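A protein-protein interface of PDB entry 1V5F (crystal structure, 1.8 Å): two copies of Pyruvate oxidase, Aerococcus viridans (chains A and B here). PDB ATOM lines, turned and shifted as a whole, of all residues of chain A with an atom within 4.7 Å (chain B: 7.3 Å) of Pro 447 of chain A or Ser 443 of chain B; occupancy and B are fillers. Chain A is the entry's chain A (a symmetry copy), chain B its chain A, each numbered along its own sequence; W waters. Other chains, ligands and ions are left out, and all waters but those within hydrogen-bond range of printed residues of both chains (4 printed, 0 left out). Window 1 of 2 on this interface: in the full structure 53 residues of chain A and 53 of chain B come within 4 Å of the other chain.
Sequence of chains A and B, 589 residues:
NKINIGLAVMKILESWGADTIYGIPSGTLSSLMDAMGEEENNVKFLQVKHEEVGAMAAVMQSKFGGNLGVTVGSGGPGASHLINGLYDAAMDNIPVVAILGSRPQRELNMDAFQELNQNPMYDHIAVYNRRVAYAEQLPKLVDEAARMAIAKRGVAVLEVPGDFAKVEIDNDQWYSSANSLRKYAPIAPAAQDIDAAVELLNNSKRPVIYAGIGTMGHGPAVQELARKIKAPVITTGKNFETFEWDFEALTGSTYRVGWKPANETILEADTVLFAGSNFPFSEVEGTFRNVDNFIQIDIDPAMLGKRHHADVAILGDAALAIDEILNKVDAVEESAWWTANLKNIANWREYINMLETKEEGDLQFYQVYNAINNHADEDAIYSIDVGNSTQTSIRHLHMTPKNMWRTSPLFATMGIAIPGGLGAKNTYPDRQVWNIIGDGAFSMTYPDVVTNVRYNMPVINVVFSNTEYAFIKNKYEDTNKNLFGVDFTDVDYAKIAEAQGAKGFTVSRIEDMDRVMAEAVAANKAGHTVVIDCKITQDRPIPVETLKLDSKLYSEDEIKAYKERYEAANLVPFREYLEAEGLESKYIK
OH of Tyr 446 of chain B lies within hydrogen-bond range of NE2 of Gln 500 of chain A, 3.0 Å away.
Water W4 lies within hydrogen-bond range of the backbone carbonyl oxygen (O) of Gly 440 of chain B and the backbone carbonyl oxygen (O) of Lys 49 of chain A. Water W1 bridges the side-chain hydroxyl of Tyr 446 of chain A (2.6 Å) and the backbone carbonyl oxygen of Pro 447 of chain B (2.7 Å). Water W2 lies within hydrogen-bond range of the side-chain hydroxyl of Tyr 446 of chain B (2.6 Å), the backbone carbonyl oxygen of Pro 447 of chain A (2.7 Å) and the side-chain amide nitrogen of Gln 500 of chain A (3.4 Å). Water W3 lies within hydrogen-bond range of NZ of Lys 49 of chain A, O of Asp 439 of chain B, OG of Ser 443 of chain B and N of Gly 440 of chain B.
O of Tyr 446 of chain A is in hydrogen-bond range of NE2 of Gln 500 of chain A (2.9 Å). OD1 of Asp 448 of chain A sits at hydrogen-bond distance from N of Lys 49 of chain A (2.8 Å). The backbone carbonyl oxygen (O) of Asp 439 of chain B is in hydrogen-bond range of the side-chain hydroxyl (OG) of Ser 443 of chain B, at 2.8 Å. The side-chain hydroxyl (OH) of Tyr 493 of chain B sits at hydrogen-bond distance from the side-chain hydroxyl (OG) of Ser 443 of chain B (3.3 Å).
Among the printed residues, pairs that only touch across the chains: Lys 49 of chain A with Ser 443 of chain B (3.6 Å), Lys 49 of chain A with Met 444 of chain B (3.3 Å), Lys 49 of chain A with Phe 488 of chain B (3.3 Å), Tyr 446 of chain A with Tyr 446 of chain B (3.5 Å), Tyr 446 of chain A with Pro 447 of chain B (3.4 Å), Pro 447 of chain A with Ser 443 of chain B (3.1 Å), Pro 447 of chain A with Tyr 446 of chain B (3.4 Å), Pro 447 of chain A with Pro 447 of chain B (3.4 Å) and Val 450 of chain A with Val 491 of chain B (3.6 Å).
Tyr 446 of chain B touches its own counterpart, Tyr 446 of chain A. Tyr 446 of chain A touches Pro 447 of chain B, and with the chains exchanged Pro 447 of chain A touches Tyr 446 of chain B. Pro 447 of chain B touches its own counterpart, Pro 447 of chain A.
Hydrophobic or aromatic side chains of chain A within 4 Å of the printed part of chain B: Tyr 446, Pro 447 and Val 450. Printed residues of chain B that touch a printed residue of chain A: Ser 443, Met 444, Tyr 446, Pro 447, Phe 488 and Val 491. Hydrophobic or aromatic side chains of chain B that line the printed part of chain A: Met 444, Tyr 446, Pro 447, Phe 488 and Val 491.
Pro 447 of chain A touches just these residues of chain B: Ser 443 (3.1 Å), Tyr 446 (3.4 Å) and Pro 447 (3.4 Å). Ser 443 of chain B touches two residues of chain A. Printed residues of chain B within 4 Å of Gln 500 of chain A: Tyr 446. Of the printed residues of chain B, Tyr 446 of chain A touches Tyr 446 and Pro 447. Printed residues of chain A within 4 Å of Val 491 of chain B: Val 450. Printed residues of chain A within 4 Å of Pro 447 of chain B: Tyr 446 and Pro 447. Printed residues of chain A within 4 Å of Phe 488 of chain B: Lys 49. Gly 440 of chain B touches none of the printed residues of chain A. Phe 442 of chain B touches none of the printed residues of chain A.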
ATOM      1  N   LYS A  49     -27.255  16.740  24.064  1.00  0.00           N
ATOM      2  CA  LYS A  49     -27.336  16.583  22.614  1.00  0.00           C
ATOM      3  C   LYS A  49     -28.353  17.542  21.999  1.00  0.00           C
ATOM      4  O   LYS A  49     -28.279  17.859  20.812  1.00  0.00           O
ATOM      5  CB  LYS A  49     -27.707  15.143  22.247  1.00  0.00           C
ATOM      6  CG  LYS A  49     -26.772  14.076  22.820  1.00  0.00           C
ATOM      7  CD  LYS A  49     -25.306  14.399  22.584  1.00  0.00           C
ATOM      8  CE  LYS A  49     -24.981  14.552  21.112  1.00  0.00           C
ATOM      9  NZ  LYS A  49     -23.536  14.840  20.912  1.00  0.00           N
ATOM     10  N   THR A 445     -36.556  12.393  22.653  1.00  0.00           N
ATOM     11  CA  THR A 445     -35.352  12.623  23.438  1.00  0.00           C
ATOM     12  C   THR A 445     -34.316  11.507  23.558  1.00  0.00           C
ATOM     13  O   THR A 445     -33.280  11.722  24.184  1.00  0.00           O
ATOM     14  CB  THR A 445     -35.735  13.001  24.879  1.00  0.00           C
ATOM     15  OG1 THR A 445     -36.601  11.989  25.409  1.00  0.00           O
ATOM     16  CG2 THR A 445     -36.452  14.346  24.920  1.00  0.00           C
ATOM     17  N   TYR A 446     -34.542  10.335  22.970  1.00  0.00           N
ATOM     18  CA  TYR A 446     -33.555   9.280  23.167  1.00  0.00           C
ATOM     19  C   TYR A 446     -32.124   9.569  22.721  1.00  0.00           C
ATOM     20  O   TYR A 446     -31.193   8.884  23.144  1.00  0.00           O
ATOM     21  CB  TYR A 446     -34.048   7.919  22.633  1.00  0.00           C
ATOM     22  CG  TYR A 446     -34.239   7.739  21.140  1.00  0.00           C
ATOM     23  CD1 TYR A 446     -35.515   7.548  20.609  1.00  0.00           C
ATOM     24  CD2 TYR A 446     -33.147   7.636  20.278  1.00  0.00           C
ATOM     25  CE1 TYR A 446     -35.704   7.247  19.259  1.00  0.00           C
ATOM     26  CE2 TYR A 446     -33.321   7.332  18.917  1.00  0.00           C
ATOM     27  CZ  TYR A 446     -34.604   7.138  18.420  1.00  0.00           C
ATOM     28  OH  TYR A 446     -34.793   6.817  17.095  1.00  0.00           O
ATOM     29  N   PRO A 447     -31.918  10.576  21.857  1.00  0.00           N
ATOM     30  CA  PRO A 447     -30.515  10.792  21.502  1.00  0.00           C
ATOM     31  C   PRO A 447     -29.689  11.166  22.742  1.00  0.00           C
ATOM     32  O   PRO A 447     -28.485  10.930  22.789  1.00  0.00           O
ATOM     33  CB  PRO A 447     -30.591  11.930  20.489  1.00  0.00           C
ATOM     34  CG  PRO A 447     -31.868  11.625  19.763  1.00  0.00           C
ATOM     35  CD  PRO A 447     -32.812  11.264  20.906  1.00  0.00           C
ATOM     36  N   ASP A 448     -30.342  11.737  23.754  1.00  0.00           N
ATOM     37  CA  ASP A 448     -29.633  12.140  24.964  1.00  0.00           C
ATOM     38  C   ASP A 448     -29.339  11.028  25.969  1.00  0.00           C
ATOM     39  O   ASP A 448     -28.844  11.289  27.071  1.00  0.00           O
ATOM     40  CB  ASP A 448     -30.365  13.297  25.648  1.00  0.00           C
ATOM     41  CG  ASP A 448     -29.802  14.653  25.242  1.00  0.00           C
ATOM     42  OD1 ASP A 448     -28.689  14.998  25.701  1.00  0.00           O
ATOM     43  OD2 ASP A 448     -30.460  15.364  24.453  1.00  0.00           O
ATOM     44  N   VAL A 449     -29.652   9.791  25.602  1.00  0.00           N
ATOM     45  CA  VAL A 449     -29.342   8.670  26.478  1.00  0.00           C
ATOM     46  C   VAL A 449     -27.816   8.630  26.556  1.00  0.00           C
ATOM     47  O   VAL A 449     -27.242   8.277  27.582  1.00  0.00           O
ATOM     48  CB  VAL A 449     -29.858   7.329  25.888  1.00  0.00           C
ATOM     49  CG1 VAL A 449     -29.123   6.149  26.522  1.00  0.00           C
ATOM     50  CG2 VAL A 449     -31.357   7.206  26.129  1.00  0.00           C
ATOM     51  N   VAL A 450     -27.164   9.017  25.463  1.00  0.00           N
ATOM     52  CA  VAL A 450     -25.704   9.017  25.399  1.00  0.00           C
ATOM     53  C   VAL A 450     -25.101   9.987  26.417  1.00  0.00           C
ATOM     54  O   VAL A 450     -23.944   9.849  26.815  1.00  0.00           O
ATOM     55  CB  VAL A 450     -25.206   9.388  23.973  1.00  0.00           C
ATOM     56  CG1 VAL A 450     -25.261  10.897  23.767  1.00  0.00           C
ATOM     57  CG2 VAL A 450     -23.798   8.850  23.755  1.00  0.00           C
ATOM     58  N   GLN A 500     -25.417   3.404  21.549  1.00  0.00           N
ATOM     59  CA  GLN A 500     -25.070   4.603  22.304  1.00  0.00           C
ATOM     60  C   GLN A 500     -24.159   4.325  23.497  1.00  0.00           C
ATOM     61  O   GLN A 500     -23.826   5.241  24.250  1.00  0.00           O
ATOM     62  CB  GLN A 500     -26.346   5.290  22.809  1.00  0.00           C
ATOM     63  CG  GLN A 500     -27.328   5.691  21.718  1.00  0.00           C
ATOM     64  CD  GLN A 500     -28.665   6.136  22.286  1.00  0.00           C
ATOM     65  OE1 GLN A 500     -29.294   5.409  23.056  1.00  0.00           O
ATOM     66  NE2 GLN A 500     -29.105   7.330  21.907  1.00  0.00           N
ATOM     67  N   MET B 414     -29.580  24.222  13.516  1.00  0.00           N
ATOM     68  CA  MET B 414     -29.110  22.871  13.266  1.00  0.00           C
ATOM     69  C   MET B 414     -30.359  21.993  13.256  1.00  0.00           C
ATOM     70  O   MET B 414     -31.376  22.345  13.866  1.00  0.00           O
ATOM     71  CB  MET B 414     -28.165  22.419  14.383  1.00  0.00           C
ATOM     72  CG  MET B 414     -26.761  22.991  14.296  1.00  0.00           C
ATOM     73  SD  MET B 414     -25.849  22.766  15.846  1.00  0.00           S
ATOM     74  CE  MET B 414     -25.651  20.978  15.881  1.00  0.00           C
ATOM     75  N   ILE B 418     -32.723  16.812   7.853  1.00  0.00           N
ATOM     76  CA  ILE B 418     -33.739  15.766   7.767  1.00  0.00           C
ATOM     77  C   ILE B 418     -35.113  16.335   7.411  1.00  0.00           C
ATOM     78  O   ILE B 418     -35.829  15.771   6.579  1.00  0.00           O
ATOM     79  CB  ILE B 418     -33.785  14.930   9.072  1.00  0.00           C
ATOM     80  CG1 ILE B 418     -32.540  14.029   9.128  1.00  0.00           C
ATOM     81  CG2 ILE B 418     -35.057  14.087   9.121  1.00  0.00           C
ATOM     82  CD1 ILE B 418     -32.357  13.270  10.432  1.00  0.00           C
ATOM     83  N   ILE B 437     -25.397  15.983   6.768  1.00  0.00           N
ATOM     84  CA  ILE B 437     -25.449  16.363   8.177  1.00  0.00           C
ATOM     85  C   ILE B 437     -24.180  16.133   9.000  1.00  0.00           C
ATOM     86  O   ILE B 437     -23.424  15.205   8.744  1.00  0.00           O
ATOM     87  CB  ILE B 437     -26.576  15.552   8.869  1.00  0.00           C
ATOM     88  CG1 ILE B 437     -27.692  15.252   7.860  1.00  0.00           C
ATOM     89  CG2 ILE B 437     -27.108  16.306  10.072  1.00  0.00           C
ATOM     90  CD1 ILE B 437     -28.714  14.231   8.329  1.00  0.00           C
ATOM     91  N   GLY B 438     -23.970  16.982  10.005  1.00  0.00           N
ATOM     92  CA  GLY B 438     -22.837  16.814  10.900  1.00  0.00           C
ATOM     93  C   GLY B 438     -23.380  15.958  12.033  1.00  0.00           C
ATOM     94  O   GLY B 438     -24.594  15.933  12.230  1.00  0.00           O
ATOM     95  N   ASP B 439     -22.528  15.255  12.778  1.00  0.00           N
ATOM     96  CA  ASP B 439     -23.043  14.407  13.855  1.00  0.00           C
ATOM     97  C   ASP B 439     -23.768  15.171  14.959  1.00  0.00           C
ATOM     98  O   ASP B 439     -24.704  14.646  15.568  1.00  0.00           O
ATOM     99  CB  ASP B 439     -21.935  13.514  14.446  1.00  0.00           C
ATOM    100  CG  ASP B 439     -20.675  14.278  14.799  1.00  0.00           C
ATOM    101  OD1 ASP B 439     -20.700  15.510  14.726  1.00  0.00           O
ATOM    102  OD2 ASP B 439     -19.656  13.643  15.157  1.00  0.00           O
ATOM    103  N   GLY B 440     -23.354  16.407  15.214  1.00  0.00           N
ATOM    104  CA  GLY B 440     -24.018  17.200  16.234  1.00  0.00           C
ATOM    105  C   GLY B 440     -25.453  17.509  15.834  1.00  0.00           C
ATOM    106  O   GLY B 440     -26.374  17.371  16.638  1.00  0.00           O
ATOM    107  N   ALA B 441     -25.647  17.926  14.586  1.00  0.00           N
ATOM    108  CA  ALA B 441     -26.984  18.249  14.096  1.00  0.00           C
ATOM    109  C   ALA B 441     -27.800  16.973  13.939  1.00  0.00           C
ATOM    110  O   ALA B 441     -29.004  16.959  14.196  1.00  0.00           O
ATOM    111  CB  ALA B 441     -26.895  18.989  12.765  1.00  0.00           C
ATOM    112  N   PHE B 442     -27.141  15.899  13.512  1.00  0.00           N
ATOM    113  CA  PHE B 442     -27.813  14.621  13.344  1.00  0.00           C
ATOM    114  C   PHE B 442     -28.365  14.171  14.696  1.00  0.00           C
ATOM    115  O   PHE B 442     -29.481  13.657  14.780  1.00  0.00           O
ATOM    116  CB  PHE B 442     -26.831  13.573  12.811  1.00  0.00           C
ATOM    117  CG  PHE B 442     -27.480  12.280  12.397  1.00  0.00           C
ATOM    118  CD1 PHE B 442     -28.432  12.260  11.382  1.00  0.00           C
ATOM    119  CD2 PHE B 442     -27.119  11.078  13.002  1.00  0.00           C
ATOM    120  CE1 PHE B 442     -29.016  11.061  10.970  1.00  0.00           C
ATOM    121  CE2 PHE B 442     -27.697   9.870  12.598  1.00  0.00           C
ATOM    122  CZ  PHE B 442     -28.646   9.862  11.579  1.00  0.00           C
ATOM    123  N   SER B 443     -27.577  14.376  15.750  1.00  0.00           N
ATOM    124  CA  SER B 443     -27.974  13.985  17.101  1.00  0.00           C
ATOM    125  C   SER B 443     -29.206  14.731  17.620  1.00  0.00           C
ATOM    126  O   SER B 443     -29.839  14.302  18.586  1.00  0.00           O
ATOM    127  CB  SER B 443     -26.802  14.187  18.070  1.00  0.00           C
ATOM    128  OG  SER B 443     -25.738  13.295  17.761  1.00  0.00           O
ATOM    129  N   MET B 444     -29.549  15.845  16.985  1.00  0.00           N
ATOM    130  CA  MET B 444     -30.720  16.613  17.403  1.00  0.00           C
ATOM    131  C   MET B 444     -31.966  16.159  16.656  1.00  0.00           C
ATOM    132  O   MET B 444     -33.085  16.524  17.027  1.00  0.00           O
ATOM    133  CB  MET B 444     -30.524  18.105  17.121  1.00  0.00           C
ATOM    134  CG  MET B 444     -29.396  18.772  17.878  1.00  0.00           C
ATOM    135  SD  MET B 444     -29.269  20.523  17.418  1.00  0.00           S
ATOM    136  CE  MET B 444     -27.945  21.073  18.545  1.00  0.00           C
ATOM    137  N   THR B 445     -31.778  15.355  15.613  1.00  0.00           N
ATOM    138  CA  THR B 445     -32.906  14.930  14.798  1.00  0.00           C
ATOM    139  C   THR B 445     -32.952  13.495  14.277  1.00  0.00           C
ATOM    140  O   THR B 445     -33.929  13.129  13.627  1.00  0.00           O
ATOM    141  CB  THR B 445     -33.021  15.834  13.558  1.00  0.00           C
ATOM    142  OG1 THR B 445     -31.764  15.837  12.870  1.00  0.00           O
ATOM    143  CG2 THR B 445     -33.381  17.262  13.953  1.00  0.00           C
ATOM    144  N   TYR B 446     -31.948  12.665  14.551  1.00  0.00           N
ATOM    145  CA  TYR B 446     -32.006  11.326  13.977  1.00  0.00           C
ATOM    146  C   TYR B 446     -33.214  10.463  14.334  1.00  0.00           C
ATOM    147  O   TYR B 446     -33.498   9.481  13.648  1.00  0.00           O
ATOM    148  CB  TYR B 446     -30.685  10.554  14.176  1.00  0.00           C
ATOM    149  CG  TYR B 446     -30.268  10.155  15.578  1.00  0.00           C
ATOM    150  CD1 TYR B 446     -29.139  10.722  16.168  1.00  0.00           C
ATOM    151  CD2 TYR B 446     -30.923   9.131  16.264  1.00  0.00           C
ATOM    152  CE1 TYR B 446     -28.659  10.275  17.401  1.00  0.00           C
ATOM    153  CE2 TYR B 446     -30.451   8.669  17.503  1.00  0.00           C
ATOM    154  CZ  TYR B 446     -29.318   9.247  18.061  1.00  0.00           C
ATOM    155  OH  TYR B 446     -28.828   8.793  19.264  1.00  0.00           O
ATOM    156  N   PRO B 447     -33.943  10.803  15.409  1.00  0.00           N
ATOM    157  CA  PRO B 447     -35.092   9.932  15.661  1.00  0.00           C
ATOM    158  C   PRO B 447     -36.082   9.981  14.487  1.00  0.00           C
ATOM    159  O   PRO B 447     -36.826   9.032  14.254  1.00  0.00           O
ATOM    160  CB  PRO B 447     -35.682  10.510  16.944  1.00  0.00           C
ATOM    161  CG  PRO B 447     -34.456  10.946  17.690  1.00  0.00           C
ATOM    162  CD  PRO B 447     -33.634  11.622  16.597  1.00  0.00           C
ATOM    163  N   VAL B 463     -23.720  11.410   7.123  1.00  0.00           N
ATOM    164  CA  VAL B 463     -23.333  11.985   8.411  1.00  0.00           C
ATOM    165  C   VAL B 463     -21.828  12.082   8.630  1.00  0.00           C
ATOM    166  O   VAL B 463     -21.100  11.099   8.482  1.00  0.00           O
ATOM    167  CB  VAL B 463     -23.953  11.168   9.568  1.00  0.00           C
ATOM    168  CG1 VAL B 463     -23.605  11.797  10.917  1.00  0.00           C
ATOM    169  CG2 VAL B 463     -25.462  11.090   9.387  1.00  0.00           C
ATOM    170  N   PHE B 488     -17.061  14.461  22.236  1.00  0.00           N
ATOM    171  CA  PHE B 488     -18.187  13.554  22.026  1.00  0.00           C
ATOM    172  C   PHE B 488     -17.581  12.186  21.721  1.00  0.00           C
ATOM    173  O   PHE B 488     -16.667  12.084  20.904  1.00  0.00           O
ATOM    174  CB  PHE B 488     -19.034  14.032  20.839  1.00  0.00           C
ATOM    175  CG  PHE B 488     -20.068  13.037  20.380  1.00  0.00           C
ATOM    176  CD1 PHE B 488     -21.121  12.666  21.210  1.00  0.00           C
ATOM    177  CD2 PHE B 488     -19.988  12.468  19.111  1.00  0.00           C
ATOM    178  CE1 PHE B 488     -22.081  11.744  20.783  1.00  0.00           C
ATOM    179  CE2 PHE B 488     -20.940  11.546  18.676  1.00  0.00           C
ATOM    180  CZ  PHE B 488     -21.987  11.185  19.513  1.00  0.00           C
ATOM    181  N   VAL B 491     -21.159   7.343  18.864  1.00  0.00           N
ATOM    182  CA  VAL B 491     -22.221   6.355  18.813  1.00  0.00           C
ATOM    183  C   VAL B 491     -22.290   5.767  17.407  1.00  0.00           C
ATOM    184  O   VAL B 491     -21.877   6.396  16.428  1.00  0.00           O
ATOM    185  CB  VAL B 491     -23.594   6.962  19.197  1.00  0.00           C
ATOM    186  CG1 VAL B 491     -23.423   7.975  20.322  1.00  0.00           C
ATOM    187  CG2 VAL B 491     -24.243   7.583  18.005  1.00  0.00           C
ATOM    188  N   TYR B 493     -24.114   5.282  14.491  1.00  0.00           N
ATOM    189  CA  TYR B 493     -25.275   5.744  13.728  1.00  0.00           C
ATOM    190  C   TYR B 493     -25.808   4.710  12.741  1.00  0.00           C
ATOM    191  O   TYR B 493     -27.009   4.660  12.479  1.00  0.00           O
ATOM    192  CB  TYR B 493     -24.941   7.038  12.979  1.00  0.00           C
ATOM    193  CG  TYR B 493     -24.567   8.182  13.888  1.00  0.00           C
ATOM    194  CD1 TYR B 493     -23.396   8.910  13.678  1.00  0.00           C
ATOM    195  CD2 TYR B 493     -25.367   8.522  14.978  1.00  0.00           C
ATOM    196  CE1 TYR B 493     -23.027   9.946  14.534  1.00  0.00           C
ATOM    197  CE2 TYR B 493     -25.008   9.558  15.839  1.00  0.00           C
ATOM    198  CZ  TYR B 493     -23.836  10.261  15.613  1.00  0.00           C
ATOM    199  OH  TYR B 493     -23.461  11.266  16.477  1.00  0.00           O
ATOM    200  N   ILE B 496     -27.984   2.421  14.641  1.00  0.00           N
ATOM    201  CA  ILE B 496     -29.224   3.097  14.984  1.00  0.00           C
ATOM    202  C   ILE B 496     -30.135   3.070  13.762  1.00  0.00           C
ATOM    203  O   ILE B 496     -31.327   2.790  13.871  1.00  0.00           O
ATOM    204  CB  ILE B 496     -28.956   4.553  15.406  1.00  0.00           C
ATOM    205  CG1 ILE B 496     -28.217   4.560  16.753  1.00  0.00           C
ATOM    206  CG2 ILE B 496     -30.269   5.321  15.493  1.00  0.00           C
ATOM    207  CD1 ILE B 496     -27.876   5.938  17.275  1.00  0.00           C
HETATM  208  O   HOH W   1     -36.991   6.793  15.681  1.00  0.00           O
HETATM  209  O   HOH W   2     -27.030   9.850  20.841  1.00  0.00           O
HETATM  210  O   HOH W   3     -22.724  14.583  17.994  1.00  0.00           O
HETATM  211  O   HOH W   4     -26.176  17.534  19.207  1.00  0.00           O
